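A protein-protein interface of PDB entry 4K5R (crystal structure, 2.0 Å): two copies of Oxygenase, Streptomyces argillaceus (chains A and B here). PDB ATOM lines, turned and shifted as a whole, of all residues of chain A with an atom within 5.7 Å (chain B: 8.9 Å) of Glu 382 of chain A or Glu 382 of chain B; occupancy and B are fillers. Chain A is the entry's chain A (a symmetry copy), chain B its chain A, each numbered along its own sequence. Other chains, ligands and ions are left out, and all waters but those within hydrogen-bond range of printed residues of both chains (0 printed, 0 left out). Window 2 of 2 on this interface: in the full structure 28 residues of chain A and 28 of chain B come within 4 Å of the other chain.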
ATOM      1  N   THR A 380       6.853   8.158  21.792  1.00  0.00           N
ATOM      2  CA  THR A 380       7.017   7.260  20.655  1.00  0.00           C
ATOM      3  C   THR A 380       7.837   7.958  19.563  1.00  0.00           C
ATOM      4  O   THR A 380       7.640   9.154  19.295  1.00  0.00           O
ATOM      5  CB  THR A 380       5.659   6.781  20.072  1.00  0.00           C
ATOM      6  OG1 THR A 380       5.020   7.855  19.366  1.00  0.00           O
ATOM      7  CG2 THR A 380       4.739   6.244  21.176  1.00  0.00           C
ATOM      8  N   ASP A 381       8.748   7.210  18.936  1.00  0.00           N
ATOM      9  CA  ASP A 381       9.630   7.778  17.913  1.00  0.00           C
ATOM     10  C   ASP A 381       8.871   8.396  16.751  1.00  0.00           C
ATOM     11  O   ASP A 381       9.253   9.465  16.259  1.00  0.00           O
ATOM     12  CB  ASP A 381      10.606   6.726  17.363  1.00  0.00           C
ATOM     13  CG  ASP A 381      11.631   6.273  18.392  1.00  0.00           C
ATOM     14  OD1 ASP A 381      11.767   6.939  19.445  1.00  0.00           O
ATOM     15  OD2 ASP A 381      12.300   5.245  18.139  1.00  0.00           O
ATOM     16  N   GLU A 382       7.813   7.727  16.291  1.00  0.00           N
ATOM     17  CA  GLU A 382       7.100   8.188  15.096  1.00  0.00           C
ATOM     18  C   GLU A 382       6.467   9.566  15.338  1.00  0.00           C
ATOM     19  O   GLU A 382       6.663  10.499  14.552  1.00  0.00           O
ATOM     20  CB  GLU A 382       6.045   7.168  14.640  1.00  0.00           C
ATOM     21  CG  GLU A 382       5.418   7.483  13.276  1.00  0.00           C
ATOM     22  CD  GLU A 382       4.129   6.700  12.991  1.00  0.00           C
ATOM     23  OE1 GLU A 382       3.970   5.568  13.509  1.00  0.00           O
ATOM     24  OE2 GLU A 382       3.266   7.222  12.242  1.00  0.00           O
ATOM     25  N   VAL A 383       5.729   9.698  16.440  1.00  0.00           N
ATOM     26  CA  VAL A 383       5.097  10.973  16.742  1.00  0.00           C
ATOM     27  C   VAL A 383       6.128  12.037  17.081  1.00  0.00           C
ATOM     28  O   VAL A 383       5.984  13.201  16.705  1.00  0.00           O
ATOM     29  CB  VAL A 383       4.112  10.870  17.903  1.00  0.00           C
ATOM     30  CG1 VAL A 383       3.567  12.256  18.243  1.00  0.00           C
ATOM     31  CG2 VAL A 383       2.991   9.909  17.545  1.00  0.00           C
ATOM     32  N   ASN A 384       7.166  11.636  17.804  1.00  0.00           N
ATOM     33  CA  ASN A 384       8.222  12.564  18.175  1.00  0.00           C
ATOM     34  C   ASN A 384       8.931  13.099  16.924  1.00  0.00           C
ATOM     35  O   ASN A 384       9.188  14.295  16.793  1.00  0.00           O
ATOM     36  CB  ASN A 384       9.208  11.866  19.103  1.00  0.00           C
ATOM     37  CG  ASN A 384      10.168  12.820  19.758  1.00  0.00           C
ATOM     38  OD1 ASN A 384      10.855  13.605  19.090  1.00  0.00           O
ATOM     39  ND2 ASN A 384      10.228  12.762  21.083  1.00  0.00           N
ATOM     40  N   ARG A 385       9.218  12.201  15.994  1.00  0.00           N
ATOM     41  CA  ARG A 385       9.822  12.589  14.731  1.00  0.00           C
ATOM     42  C   ARG A 385       8.883  13.543  14.006  1.00  0.00           C
ATOM     43  O   ARG A 385       9.324  14.486  13.348  1.00  0.00           O
ATOM     44  CB  ARG A 385      10.092  11.353  13.866  1.00  0.00           C
ATOM     45  CG  ARG A 385      10.631  11.662  12.472  1.00  0.00           C
ATOM     46  CD  ARG A 385      11.040  10.384  11.749  1.00  0.00           C
ATOM     47  NE  ARG A 385      11.920   9.564  12.583  1.00  0.00           N
ATOM     48  CZ  ARG A 385      11.540   8.462  13.220  1.00  0.00           C
ATOM     49  NH1 ARG A 385      10.289   8.030  13.110  1.00  0.00           N
ATOM     50  NH2 ARG A 385      12.413   7.789  13.963  1.00  0.00           N
ATOM     51  N   TYR A 386       7.582  13.301  14.142  1.00  0.00           N
ATOM     52  CA  TYR A 386       6.581  14.132  13.481  1.00  0.00           C
ATOM     53  C   TYR A 386       6.727  15.593  13.910  1.00  0.00           C
ATOM     54  O   TYR A 386       6.895  16.488  13.072  1.00  0.00           O
ATOM     55  CB  TYR A 386       5.176  13.601  13.768  1.00  0.00           C
ATOM     56  CG  TYR A 386       4.030  14.446  13.236  1.00  0.00           C
ATOM     57  CD1 TYR A 386       3.861  14.664  11.871  1.00  0.00           C
ATOM     58  CD2 TYR A 386       3.090  14.994  14.108  1.00  0.00           C
ATOM     59  CE1 TYR A 386       2.797  15.421  11.393  1.00  0.00           C
ATOM     60  CE2 TYR A 386       2.029  15.751  13.643  1.00  0.00           C
ATOM     61  CZ  TYR A 386       1.883  15.960  12.292  1.00  0.00           C
ATOM     62  OH  TYR A 386       0.817  16.716  11.856  1.00  0.00           O
ATOM     63  N   PHE A 387       6.698  15.826  15.221  1.00  0.00           N
ATOM     64  CA  PHE A 387       6.799  17.185  15.758  1.00  0.00           C
ATOM     65  C   PHE A 387       8.196  17.778  15.630  1.00  0.00           C
ATOM     66  O   PHE A 387       8.344  18.971  15.339  1.00  0.00           O
ATOM     67  CB  PHE A 387       6.301  17.228  17.199  1.00  0.00           C
ATOM     68  CG  PHE A 387       4.826  17.065  17.302  1.00  0.00           C
ATOM     69  CD1 PHE A 387       3.984  18.040  16.786  1.00  0.00           C
ATOM     70  CD2 PHE A 387       4.274  15.936  17.876  1.00  0.00           C
ATOM     71  CE1 PHE A 387       2.621  17.900  16.856  1.00  0.00           C
ATOM     72  CE2 PHE A 387       2.909  15.788  17.954  1.00  0.00           C
ATOM     73  CZ  PHE A 387       2.081  16.769  17.443  1.00  0.00           C
ATOM     74  N   LEU B 100      -7.876  -2.213  13.057  1.00  0.00           N
ATOM     75  CA  LEU B 100      -6.475  -2.174  13.444  1.00  0.00           C
ATOM     76  C   LEU B 100      -6.256  -2.887  14.762  1.00  0.00           C
ATOM     77  O   LEU B 100      -5.123  -3.042  15.207  1.00  0.00           O
ATOM     78  CB  LEU B 100      -5.990  -0.729  13.560  1.00  0.00           C
ATOM     79  CG  LEU B 100      -6.058   0.115  12.288  1.00  0.00           C
ATOM     80  CD1 LEU B 100      -5.893   1.594  12.628  1.00  0.00           C
ATOM     81  CD2 LEU B 100      -5.014  -0.351  11.280  1.00  0.00           C
ATOM     82  N   VAL B 101      -7.342  -3.305  15.400  1.00  0.00           N
ATOM     83  CA  VAL B 101      -7.215  -3.990  16.678  1.00  0.00           C
ATOM     84  C   VAL B 101      -7.515  -5.485  16.550  1.00  0.00           C
ATOM     85  O   VAL B 101      -8.279  -5.912  15.677  1.00  0.00           O
ATOM     86  CB  VAL B 101      -8.098  -3.349  17.781  1.00  0.00           C
ATOM     87  CG1 VAL B 101      -7.810  -1.849  17.891  1.00  0.00           C
ATOM     88  CG2 VAL B 101      -9.574  -3.617  17.518  1.00  0.00           C
ATOM     89  N   GLU B 376      -4.602  14.707  11.478  1.00  0.00           N
ATOM     90  CA  GLU B 376      -3.499  14.138  10.702  1.00  0.00           C
ATOM     91  C   GLU B 376      -2.997  12.885  11.390  1.00  0.00           C
ATOM     92  O   GLU B 376      -2.836  11.845  10.760  1.00  0.00           O
ATOM     93  CB  GLU B 376      -2.341  15.133  10.546  1.00  0.00           C
ATOM     94  CG  GLU B 376      -2.592  16.236   9.536  1.00  0.00           C
ATOM     95  CD  GLU B 376      -1.441  17.238   9.445  1.00  0.00           C
ATOM     96  OE1 GLU B 376      -0.268  16.816   9.564  1.00  0.00           O
ATOM     97  OE2 GLU B 376      -1.717  18.449   9.251  1.00  0.00           O
ATOM     98  N   LEU B 377      -2.776  12.988  12.696  1.00  0.00           N
ATOM     99  CA  LEU B 377      -2.203  11.899  13.466  1.00  0.00           C
ATOM    100  C   LEU B 377      -3.110  10.676  13.472  1.00  0.00           C
ATOM    101  O   LEU B 377      -2.627   9.549  13.363  1.00  0.00           O
ATOM    102  CB  LEU B 377      -1.886  12.346  14.894  1.00  0.00           C
ATOM    103  CG  LEU B 377      -0.737  13.349  14.992  1.00  0.00           C
ATOM    104  CD1 LEU B 377      -0.540  13.832  16.417  1.00  0.00           C
ATOM    105  CD2 LEU B 377       0.542  12.728  14.452  1.00  0.00           C
ATOM    106  N   LEU B 378      -4.417  10.895  13.582  1.00  0.00           N
ATOM    107  CA  LEU B 378      -5.378   9.790  13.546  1.00  0.00           C
ATOM    108  C   LEU B 378      -5.368   9.058  12.192  1.00  0.00           C
ATOM    109  O   LEU B 378      -5.878   7.942  12.065  1.00  0.00           O
ATOM    110  CB  LEU B 378      -6.783  10.294  13.866  1.00  0.00           C
ATOM    111  CG  LEU B 378      -7.057  10.590  15.335  1.00  0.00           C
ATOM    112  CD1 LEU B 378      -8.330  11.405  15.442  1.00  0.00           C
ATOM    113  CD2 LEU B 378      -7.155   9.278  16.133  1.00  0.00           C
ATOM    114  N   GLY B 379      -4.789   9.699  11.186  1.00  0.00           N
ATOM    115  CA  GLY B 379      -4.644   9.088   9.881  1.00  0.00           C
ATOM    116  C   GLY B 379      -3.519   8.070   9.843  1.00  0.00           C
ATOM    117  O   GLY B 379      -3.373   7.338   8.863  1.00  0.00           O
ATOM    118  N   THR B 380      -2.709   8.034  10.896  1.00  0.00           N
ATOM    119  CA  THR B 380      -1.665   7.022  10.995  1.00  0.00           C
ATOM    120  C   THR B 380      -2.176   5.835  11.821  1.00  0.00           C
ATOM    121  O   THR B 380      -2.856   6.025  12.843  1.00  0.00           O
ATOM    122  CB  THR B 380      -0.354   7.574  11.618  1.00  0.00           C
ATOM    123  OG1 THR B 380      -0.531   7.792  13.026  1.00  0.00           O
ATOM    124  CG2 THR B 380       0.085   8.871  10.927  1.00  0.00           C
ATOM    125  N   ASP B 381      -1.846   4.619  11.381  1.00  0.00           N
ATOM    126  CA  ASP B 381      -2.321   3.408  12.054  1.00  0.00           C
ATOM    127  C   ASP B 381      -1.909   3.339  13.515  1.00  0.00           C
ATOM    128  O   ASP B 381      -2.709   2.931  14.366  1.00  0.00           O
ATOM    129  CB  ASP B 381      -1.829   2.137  11.342  1.00  0.00           C
ATOM    130  CG  ASP B 381      -2.450   1.951   9.965  1.00  0.00           C
ATOM    131  OD1 ASP B 381      -3.445   2.645   9.651  1.00  0.00           O
ATOM    132  OD2 ASP B 381      -1.934   1.104   9.200  1.00  0.00           O
ATOM    133  N   GLU B 382      -0.665   3.714  13.814  1.00  0.00           N
ATOM    134  CA  GLU B 382      -0.148   3.561  15.178  1.00  0.00           C
ATOM    135  C   GLU B 382      -0.939   4.437  16.160  1.00  0.00           C
ATOM    136  O   GLU B 382      -1.421   3.955  17.191  1.00  0.00           O
ATOM    137  CB  GLU B 382       1.356   3.873  15.248  1.00  0.00           C
ATOM    138  CG  GLU B 382       2.004   3.522  16.593  1.00  0.00           C
ATOM    139  CD  GLU B 382       3.386   4.160  16.800  1.00  0.00           C
ATOM    140  OE1 GLU B 382       4.104   4.407  15.800  1.00  0.00           O
ATOM    141  OE2 GLU B 382       3.756   4.418  17.972  1.00  0.00           O
ATOM    142  N   VAL B 383      -1.095   5.718  15.826  1.00  0.00           N
ATOM    143  CA  VAL B 383      -1.834   6.613  16.703  1.00  0.00           C
ATOM    144  C   VAL B 383      -3.310   6.252  16.746  1.00  0.00           C
ATOM    145  O   VAL B 383      -3.950   6.328  17.796  1.00  0.00           O
ATOM    146  CB  VAL B 383      -1.707   8.073  16.280  1.00  0.00           C
ATOM    147  CG1 VAL B 383      -2.591   8.947  17.169  1.00  0.00           C
ATOM    148  CG2 VAL B 383      -0.253   8.507  16.352  1.00  0.00           C
ATOM    149  N   ASN B 384      -3.853   5.869  15.598  1.00  0.00           N
ATOM    150  CA  ASN B 384      -5.253   5.487  15.523  1.00  0.00           C
ATOM    151  C   ASN B 384      -5.520   4.252  16.394  1.00  0.00           C
ATOM    152  O   ASN B 384      -6.494   4.191  17.142  1.00  0.00           O
ATOM    153  CB  ASN B 384      -5.629   5.221  14.071  1.00  0.00           C
ATOM    154  CG  ASN B 384      -7.114   5.097  13.867  1.00  0.00           C
ATOM    155  OD1 ASN B 384      -7.792   4.297  14.527  1.00  0.00           O
ATOM    156  ND2 ASN B 384      -7.639   5.891  12.942  1.00  0.00           N
ATOM    157  N   ARG B 385      -4.625   3.279  16.308  1.00  0.00           N
ATOM    158  CA  ARG B 385      -4.721   2.090  17.134  1.00  0.00           C
ATOM    159  C   ARG B 385      -4.643   2.496  18.599  1.00  0.00           C
ATOM    160  O   ARG B 385      -5.312   1.915  19.454  1.00  0.00           O
ATOM    161  CB  ARG B 385      -3.592   1.111  16.795  1.00  0.00           C
ATOM    162  CG  ARG B 385      -3.541  -0.130  17.684  1.00  0.00           C
ATOM    163  CD  ARG B 385      -2.511  -1.128  17.169  1.00  0.00           C
ATOM    164  NE  ARG B 385      -2.702  -1.397  15.744  1.00  0.00           N
ATOM    165  CZ  ARG B 385      -1.938  -0.903  14.776  1.00  0.00           C
ATOM    166  NH1 ARG B 385      -0.910  -0.118  15.078  1.00  0.00           N
ATOM    167  NH2 ARG B 385      -2.198  -1.199  13.506  1.00  0.00           N
ATOM    168  N   TYR B 386      -3.830   3.510  18.882  1.00  0.00           N
ATOM    169  CA  TYR B 386      -3.653   3.983  20.252  1.00  0.00           C
ATOM    170  C   TYR B 386      -4.993   4.412  20.850  1.00  0.00           C
ATOM    171  O   TYR B 386      -5.410   3.910  21.902  1.00  0.00           O
ATOM    172  CB  TYR B 386      -2.630   5.119  20.294  1.00  0.00           C
ATOM    173  CG  TYR B 386      -2.439   5.785  21.647  1.00  0.00           C
ATOM    174  CD1 TYR B 386      -1.959   5.075  22.744  1.00  0.00           C
ATOM    175  CD2 TYR B 386      -2.705   7.144  21.811  1.00  0.00           C
ATOM    176  CE1 TYR B 386      -1.768   5.698  23.973  1.00  0.00           C
ATOM    177  CE2 TYR B 386      -2.520   7.774  23.030  1.00  0.00           C
ATOM    178  CZ  TYR B 386      -2.052   7.054  24.104  1.00  0.00           C
ATOM    179  OH  TYR B 386      -1.875   7.706  25.304  1.00  0.00           O
ATOM    180  N   PHE B 387      -5.683   5.316  20.157  1.00  0.00           N
ATOM    181  CA  PHE B 387      -6.968   5.830  20.637  1.00  0.00           C
ATOM    182  C   PHE B 387      -8.097   4.812  20.535  1.00  0.00           C
ATOM    183  O   PHE B 387      -8.947   4.730  21.430  1.00  0.00           O
ATOM    184  CB  PHE B 387      -7.321   7.133  19.929  1.00  0.00           C
ATOM    185  CG  PHE B 387      -6.462   8.270  20.355  1.00  0.00           C
ATOM    186  CD1 PHE B 387      -6.535   8.743  21.657  1.00  0.00           C
ATOM    187  CD2 PHE B 387      -5.561   8.847  19.480  1.00  0.00           C
ATOM    188  CE1 PHE B 387      -5.739   9.779  22.074  1.00  0.00           C
ATOM    189  CE2 PHE B 387      -4.761   9.888  19.888  1.00  0.00           C
ATOM    190  CZ  PHE B 387      -4.847  10.355  21.186  1.00  0.00           C
ATOM    191  N   THR B 388      -8.097   4.019  19.464  1.00  0.00           N
ATOM    192  CA  THR B 388      -9.093   2.968  19.341  1.00  0.00           C
ATOM    193  C   THR B 388      -9.031   2.067  20.557  1.00  0.00           C
ATOM    194  O   THR B 388     -10.045   1.798  21.190  1.00  0.00           O
ATOM    195  CB  THR B 388      -8.897   2.117  18.081  1.00  0.00           C
ATOM    196  OG1 THR B 388      -9.106   2.934  16.925  1.00  0.00           O
ATOM    197  CG2 THR B 388      -9.907   0.982  18.072  1.00  0.00           C
ATOM    198  N   GLY B 389      -7.829   1.610  20.887  1.00  0.00           N
ATOM    199  CA  GLY B 389      -7.645   0.725  22.021  1.00  0.00           C
ATOM    200  C   GLY B 389      -8.110   1.350  23.318  1.00  0.00           C
ATOM    201  O   GLY B 389      -8.661   0.676  24.191  1.00  0.00           O
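O of Leu 377 of chain B lies within hydrogen-bond range of OG1 of Thr 380 of chain B (2.8 Å).
The side-chain hydroxyl (OH) of Tyr 386 of chain A lies within hydrogen-bond range of the side-chain carboxylate (OE1) of Glu 376 of chain B, 2.5 Å away. The side-chain carboxylate of Glu 382 of chain A sits close to the side-chain carboxylate of Glu 382 of chain B, at 2.6 Å.
Thr 380 of chain A touches Glu 382 of chain B, and with the chains exchanged Glu 382 of chain A touches Thr 380 of chain B. Glu 382 of chain A touches its own counterpart, Glu 382 of chain B. Val 383 of chain B touches its own counterpart, Val 383 of chain A. Positions printed for both chains: 380, 381, 382, 383, 384, 385, 386 and 387. Of the 6 pairs that touch across the chains among the printed residues, 4 have their exchanged pair printed and touching as well.
Of the printed residues of chain B, Thr 380 of chain A touches Glu 382 (3.7 Å). Glu 382 of chain A touches two residues of chain B. Of the printed residues of chain A, Glu 376 of chain B touches Tyr 386. Of the printed residues of chain A, Leu 377 of chain B touches Tyr 386 (3.4 Å). Of the printed residues of chain A, Thr 380 of chain B touches Glu 382. Glu 382 of chain B touches just these residues of chain A: Thr 380 (3.7 Å) and Glu 382 (2.6 Å). Of the printed residues of chain A, Val 383 of chain B touches Val 383 (3.7 Å). The nearest printed residue of chain B that does not touch Tyr 386 of chain A is Thr 380 of chain B (7.0 Å).
Of the 8 printed residues of chain A, 4 touch a printed residue of chain B. Printed residues of chain A that touch a printed residue of chain B: Thr 380, Glu 382, Val 383 and Tyr 386. Hydrophobic or aromatic side chains of chain A that line the printed part of chain B: Val 383 and Tyr 386. Printed residues of chain B that touch a printed residue of chain A: Glu 376, Leu 377, Thr 380, Glu 382 and Val 383. Among the printed residues, 6 pairs touch across the chains.
Among the printed residues, merely in contact across the chains: Thr 380 of chain A with Glu 382 of chain B, Glu 382 of chain A with Thr 380 of chain B, Val 383 of chain A with Val 383 of chain B and Tyr 386 of chain A with Leu 377 of chain B.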
